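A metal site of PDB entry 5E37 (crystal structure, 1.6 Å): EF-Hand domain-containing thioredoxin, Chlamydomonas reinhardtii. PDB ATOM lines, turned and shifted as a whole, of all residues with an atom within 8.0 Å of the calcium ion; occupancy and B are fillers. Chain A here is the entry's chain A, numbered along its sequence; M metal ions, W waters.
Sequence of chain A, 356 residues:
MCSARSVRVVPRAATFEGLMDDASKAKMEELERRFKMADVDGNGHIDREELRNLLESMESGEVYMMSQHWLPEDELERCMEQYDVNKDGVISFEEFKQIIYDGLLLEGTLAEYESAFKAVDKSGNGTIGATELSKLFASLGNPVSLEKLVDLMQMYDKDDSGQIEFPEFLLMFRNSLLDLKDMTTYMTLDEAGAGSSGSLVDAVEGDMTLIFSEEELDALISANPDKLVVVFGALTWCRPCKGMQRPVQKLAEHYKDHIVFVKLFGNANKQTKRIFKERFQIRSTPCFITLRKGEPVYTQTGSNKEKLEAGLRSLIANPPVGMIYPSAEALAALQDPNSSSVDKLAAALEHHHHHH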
ATOM      1  N   PHE A 117     -31.899  -4.984  -6.157  1.00  0.00           N
ATOM      2  CA  PHE A 117     -31.135  -4.999  -7.408  1.00  0.00           C
ATOM      3  C   PHE A 117     -31.852  -4.224  -8.477  1.00  0.00           C
ATOM      4  O   PHE A 117     -31.214  -3.466  -9.252  1.00  0.00           O
ATOM      5  CB  PHE A 117     -31.001  -6.437  -7.864  1.00  0.00           C
ATOM      6  CG  PHE A 117     -30.201  -6.612  -9.069  1.00  0.00           C
ATOM      7  CD1 PHE A 117     -28.874  -6.771  -8.992  1.00  0.00           C
ATOM      8  CD2 PHE A 117     -30.818  -6.676 -10.297  1.00  0.00           C
ATOM      9  CE1 PHE A 117     -28.093  -6.955 -10.137  1.00  0.00           C
ATOM     10  CE2 PHE A 117     -30.049  -6.833 -11.449  1.00  0.00           C
ATOM     11  CZ  PHE A 117     -28.668  -7.008 -11.359  1.00  0.00           C
ATOM     12  N   LYS A 118     -33.156  -4.463  -8.560  1.00  0.00           N
ATOM     13  CA  LYS A 118     -34.010  -3.778  -9.535  1.00  0.00           C
ATOM     14  C   LYS A 118     -34.052  -2.243  -9.317  1.00  0.00           C
ATOM     15  O   LYS A 118     -34.015  -1.440 -10.294  1.00  0.00           O
ATOM     16  CB  LYS A 118     -35.419  -4.379  -9.592  1.00  0.00           C
ATOM     17  CG  LYS A 118     -35.420  -5.770 -10.164  1.00  0.00           C
ATOM     18  CD  LYS A 118     -36.865  -6.286 -10.243  1.00  0.00           C
ATOM     19  CE  LYS A 118     -36.887  -7.717 -10.678  1.00  0.00           C
ATOM     20  NZ  LYS A 118     -37.815  -7.842 -11.839  1.00  0.00           N
ATOM     21  N   VAL A 120     -31.569  -0.423  -8.076  1.00  0.00           N
ATOM     22  CA  VAL A 120     -30.276   0.078  -8.487  1.00  0.00           C
ATOM     23  C   VAL A 120     -30.088   0.066 -10.000  1.00  0.00           C
ATOM     24  O   VAL A 120     -29.449   0.955 -10.603  1.00  0.00           O
ATOM     25  CB  VAL A 120     -29.098  -0.676  -7.823  1.00  0.00           C
ATOM     26  CG1 VAL A 120     -27.743  -0.123  -8.284  1.00  0.00           C
ATOM     27  CG2 VAL A 120     -29.197  -0.584  -6.308  1.00  0.00           C
ATOM     28  N   ASP A 121     -30.691  -0.954 -10.628  1.00  0.00           N
ATOM     29  CA  ASP A 121     -30.641  -1.082 -12.083  1.00  0.00           C
ATOM     30  C   ASP A 121     -31.634  -0.176 -12.700  1.00  0.00           C
ATOM     31  O   ASP A 121     -32.718  -0.590 -13.175  1.00  0.00           O
ATOM     32  CB  ASP A 121     -30.942  -2.547 -12.490  1.00  0.00           C
ATOM     33  CG  ASP A 121     -31.003  -2.730 -13.977  1.00  0.00           C
ATOM     34  OD1 ASP A 121     -30.460  -1.897 -14.731  1.00  0.00           O
ATOM     35  OD2 ASP A 121     -31.608  -3.739 -14.368  1.00  0.00           O
ATOM     36  N   LYS A 122     -31.229   1.081 -12.835  1.00  0.00           N
ATOM     37  CA  LYS A 122     -32.155   2.090 -13.334  1.00  0.00           C
ATOM     38  C   LYS A 122     -32.471   1.889 -14.771  1.00  0.00           C
ATOM     39  O   LYS A 122     -33.630   2.228 -15.161  1.00  0.00           O
ATOM     40  CB  LYS A 122     -31.548   3.504 -13.140  1.00  0.00           C
ATOM     41  CG  LYS A 122     -31.532   4.008 -11.731  1.00  0.00           C
ATOM     42  CD  LYS A 122     -32.906   4.174 -11.064  1.00  0.00           C
ATOM     43  CE  LYS A 122     -32.736   4.927  -9.735  1.00  0.00           C
ATOM     44  NZ  LYS A 122     -33.547   4.324  -8.627  1.00  0.00           N
ATOM     45  N   SER A 123     -31.545   1.343 -15.575  1.00  0.00           N
ATOM     46  CA  SER A 123     -31.829   1.136 -17.036  1.00  0.00           C
ATOM     47  C   SER A 123     -32.880   0.021 -17.222  1.00  0.00           C
ATOM     48  O   SER A 123     -33.636   0.046 -18.234  1.00  0.00           O
ATOM     49  CB  SER A 123     -30.635   0.876 -17.905  1.00  0.00           C
ATOM     50  OG  SER A 123     -30.048  -0.392 -17.720  1.00  0.00           O
ATOM     51  N   GLY A 124     -32.999  -0.869 -16.245  1.00  0.00           N
ATOM     52  CA  GLY A 124     -33.951  -1.994 -16.276  1.00  0.00           C
ATOM     53  C   GLY A 124     -33.582  -3.145 -17.186  1.00  0.00           C
ATOM     54  O   GLY A 124     -34.352  -4.140 -17.312  1.00  0.00           O
ATOM     55  N   ASN A 125     -32.373  -3.130 -17.741  1.00  0.00           N
ATOM     56  CA  ASN A 125     -31.839  -4.214 -18.529  1.00  0.00           C
ATOM     57  C   ASN A 125     -31.469  -5.522 -17.819  1.00  0.00           C
ATOM     58  O   ASN A 125     -31.207  -6.485 -18.473  1.00  0.00           O
ATOM     59  CB  ASN A 125     -30.620  -3.756 -19.349  1.00  0.00           C
ATOM     60  CG  ASN A 125     -29.348  -3.662 -18.522  1.00  0.00           C
ATOM     61  OD1 ASN A 125     -29.425  -3.167 -17.418  1.00  0.00           O
ATOM     62  ND2 ASN A 125     -28.281  -4.194 -18.972  1.00  0.00           N
ATOM     63  N   GLY A 126     -31.401  -5.507 -16.476  1.00  0.00           N
ATOM     64  CA  GLY A 126     -31.155  -6.664 -15.693  1.00  0.00           C
ATOM     65  C   GLY A 126     -29.750  -6.815 -15.158  1.00  0.00           C
ATOM     66  O   GLY A 126     -29.409  -7.835 -14.506  1.00  0.00           O
ATOM     67  N   THR A 127     -28.918  -5.775 -15.422  1.00  0.00           N
ATOM     68  CA  THR A 127     -27.530  -5.759 -14.880  1.00  0.00           C
ATOM     69  C   THR A 127     -27.178  -4.366 -14.450  1.00  0.00           C
ATOM     70  O   THR A 127     -27.805  -3.408 -14.865  1.00  0.00           O
ATOM     71  CB  THR A 127     -26.438  -6.219 -15.824  1.00  0.00           C
ATOM     72  OG1 THR A 127     -26.310  -5.320 -16.915  1.00  0.00           O
ATOM     73  CG2 THR A 127     -26.798  -7.569 -16.429  1.00  0.00           C
ATOM     74  N   ILE A 128     -26.304  -4.253 -13.462  1.00  0.00           N
ATOM     75  CA  ILE A 128     -25.913  -2.921 -12.869  1.00  0.00           C
ATOM     76  C   ILE A 128     -24.585  -2.440 -13.425  1.00  0.00           C
ATOM     77  O   ILE A 128     -23.597  -3.137 -13.270  1.00  0.00           O
ATOM     78  CB  ILE A 128     -25.885  -2.986 -11.333  1.00  0.00           C
ATOM     79  CG1 ILE A 128     -27.299  -3.251 -10.771  1.00  0.00           C
ATOM     80  CG2 ILE A 128     -25.230  -1.753 -10.746  1.00  0.00           C
ATOM     81  CD1 ILE A 128     -27.316  -3.638  -9.329  1.00  0.00           C
ATOM     82  N   GLY A 129     -24.571  -1.306 -14.105  1.00  0.00           N
ATOM     83  CA  GLY A 129     -23.309  -0.768 -14.611  1.00  0.00           C
ATOM     84  C   GLY A 129     -22.719   0.230 -13.693  1.00  0.00           C
ATOM     85  O   GLY A 129     -23.359   0.560 -12.694  1.00  0.00           O
ATOM     86  N   ALA A 130     -21.515   0.635 -14.031  1.00  0.00           N
ATOM     87  CA  ALA A 130     -20.769   1.550 -13.120  1.00  0.00           C
ATOM     88  C   ALA A 130     -21.472   2.880 -12.987  1.00  0.00           C
ATOM     89  O   ALA A 130     -21.483   3.467 -11.908  1.00  0.00           O
ATOM     90  CB  ALA A 130     -19.350   1.735 -13.647  1.00  0.00           C
ATOM     91  N   GLU A 132     -24.690   3.316 -13.061  1.00  0.00           N
ATOM     92  CA  GLU A 132     -25.707   3.048 -12.052  1.00  0.00           C
ATOM     93  C   GLU A 132     -25.223   3.018 -10.635  1.00  0.00           C
ATOM     94  O   GLU A 132     -25.920   3.458  -9.728  1.00  0.00           O
ATOM     95  CB  GLU A 132     -26.474   1.756 -12.443  1.00  0.00           C
ATOM     96  CG  GLU A 132     -27.333   2.019 -13.662  1.00  0.00           C
ATOM     97  CD  GLU A 132     -27.850   0.771 -14.407  1.00  0.00           C
ATOM     98  OE1 GLU A 132     -27.337  -0.355 -14.221  1.00  0.00           O
ATOM     99  OE2 GLU A 132     -28.790   0.936 -15.220  1.00  0.00           O
ATOM    100  N   GLN A 163     -20.225  -5.435 -15.793  1.00  0.00           N
ATOM    101  CA  GLN A 163     -21.456  -5.174 -15.107  1.00  0.00           C
ATOM    102  C   GLN A 163     -21.467  -5.952 -13.810  1.00  0.00           C
ATOM    103  O   GLN A 163     -20.755  -6.986 -13.634  1.00  0.00           O
ATOM    104  CB  GLN A 163     -22.653  -5.665 -15.951  1.00  0.00           C
ATOM    105  CG  GLN A 163     -22.848  -4.971 -17.281  1.00  0.00           C
ATOM    106  CD  GLN A 163     -23.404  -3.580 -17.152  1.00  0.00           C
ATOM    107  OE1 GLN A 163     -24.495  -3.411 -16.651  1.00  0.00           O
ATOM    108  NE2 GLN A 163     -22.686  -2.603 -17.663  1.00  0.00           N
ATOM    109  N   ILE A 164     -22.270  -5.454 -12.902  1.00  0.00           N
ATOM    110  CA  ILE A 164     -22.562  -6.234 -11.646  1.00  0.00           C
ATOM    111  C   ILE A 164     -23.832  -7.029 -11.900  1.00  0.00           C
ATOM    112  O   ILE A 164     -24.911  -6.456 -12.059  1.00  0.00           O
ATOM    113  CB  ILE A 164     -22.707  -5.291 -10.471  1.00  0.00           C
ATOM    114  CG1 ILE A 164     -21.439  -4.433 -10.229  1.00  0.00           C
ATOM    115  CG2 ILE A 164     -23.078  -6.014  -9.167  1.00  0.00           C
ATOM    116  CD1 ILE A 164     -20.186  -5.185 -10.036  1.00  0.00           C
ATOM    117  N   SER A 197     -34.995   2.967 -20.010  1.00  0.00           N
ATOM    118  CA  SER A 197     -34.508   2.799 -21.305  1.00  0.00           C
ATOM    119  C   SER A 197     -34.357   1.386 -21.773  1.00  0.00           C
ATOM    120  O   SER A 197     -34.365   1.152 -22.982  1.00  0.00           O
ATOM    121  CB  SER A 197     -33.163   3.504 -21.424  1.00  0.00           C
ATOM    122  OG  SER A 197     -32.242   2.881 -20.520  1.00  0.00           O
ATOM    123  N   GLY A 198     -34.066   0.431 -20.884  1.00  0.00           N
ATOM    124  CA  GLY A 198     -33.585  -0.871 -21.281  1.00  0.00           C
ATOM    125  C   GLY A 198     -32.144  -1.025 -21.803  1.00  0.00           C
ATOM    126  O   GLY A 198     -31.742  -2.104 -22.234  1.00  0.00           O
ATOM    127  N   SER A 199     -31.385   0.058 -21.716  1.00  0.00           N
ATOM    128  CA  SER A 199     -30.022   0.127 -22.273  1.00  0.00           C
ATOM    129  C   SER A 199     -28.991  -0.560 -21.359  1.00  0.00           C
ATOM    130  O   SER A 199     -29.206  -0.720 -20.191  1.00  0.00           O
ATOM    131  CB  SER A 199     -29.556   1.597 -22.353  1.00  0.00           C
ATOM    132  OG  SER A 199     -30.489   2.337 -23.125  1.00  0.00           O
ATOM    133  N   LEU A 200     -27.916  -0.949 -21.936  1.00  0.00           N
ATOM    134  CA  LEU A 200     -26.758  -1.353 -21.174  1.00  0.00           C
ATOM    135  C   LEU A 200     -26.084  -0.146 -20.433  1.00  0.00           C
ATOM    136  O   LEU A 200     -25.624  -0.277 -19.322  1.00  0.00           O
ATOM    137  CB  LEU A 200     -25.762  -1.975 -22.137  1.00  0.00           C
ATOM    138  CG  LEU A 200     -24.495  -2.528 -21.565  1.00  0.00           C
ATOM    139  CD1 LEU A 200     -24.756  -3.649 -20.571  1.00  0.00           C
ATOM    140  CD2 LEU A 200     -23.502  -2.919 -22.653  1.00  0.00           C
ATOM    141  N   VAL A 201     -26.004   0.975 -21.119  1.00  0.00           N
ATOM    142  CA  VAL A 201     -25.501   2.228 -20.564  1.00  0.00           C
ATOM    143  C   VAL A 201     -26.191   3.425 -21.126  1.00  0.00           C
ATOM    144  O   VAL A 201     -26.402   3.446 -22.316  1.00  0.00           O
ATOM    145  CB  VAL A 201     -23.978   2.275 -20.756  1.00  0.00           C
ATOM    146  CG1 VAL A 201     -23.599   2.290 -22.208  1.00  0.00           C
ATOM    147  CG2 VAL A 201     -23.445   3.489 -19.992  1.00  0.00           C
ATOM    148  N   ASP A 202     -26.569   4.348 -20.249  1.00  0.00           N
ATOM    149  CA  ASP A 202     -27.125   5.615 -20.635  1.00  0.00           C
ATOM    150  C   ASP A 202     -26.193   6.722 -20.128  1.00  0.00           C
ATOM    151  O   ASP A 202     -26.006   6.862 -18.931  1.00  0.00           O
ATOM    152  CB  ASP A 202     -28.479   5.822 -20.065  1.00  0.00           C
ATOM    153  CG  ASP A 202     -29.535   4.977 -20.776  1.00  0.00           C
ATOM    154  OD1 ASP A 202     -29.739   5.125 -22.019  1.00  0.00           O
ATOM    155  OD2 ASP A 202     -30.044   4.181 -20.043  1.00  0.00           O
HETATM  156 CA    CA M   1     -28.635  -1.401 -15.963  1.00  0.00          CA
HETATM  157  O   HOH W   1     -26.491  -1.575 -17.117  1.00  0.00           O
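OD1 of Asp 121 lies close to N of Gly 124.
The side-chain carboxylate of Asp 121 lies within hydrogen-bond range of the backbone NH of Gly 126 (2.8 Å).
N of Gly 129 lies close to OE1 of Glu 132, 2.9 Å away.
N of Lys 122 lies close to OE2 of Glu 132, at 3.4 Å.
The side-chain hydroxyl (OG1) of Thr 127 lies within hydrogen-bond range of the side-chain amide oxygen (OE1) of Gln 163, at 2.6 Å.
O of Ser 199 sits close to OG of Ser 123, at 2.6 Å.
N of Gly 198 is in hydrogen-bond range of O of Ser 123 (2.7 Å).
Water W1 bridges O of Leu 200 and OE1 of Gln 163.
The calcium ion is bound by OD1 of Asp 121 (2.3 Å), OE1 of Glu 132 (2.4 Å), OD1 of Asn 125 (2.4 Å), O of Thr 127 (2.4 Å), water W1 (2.4 Å), OE2 of Glu 132 (2.5 Å) and OG of Ser 123 (2.5 Å).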
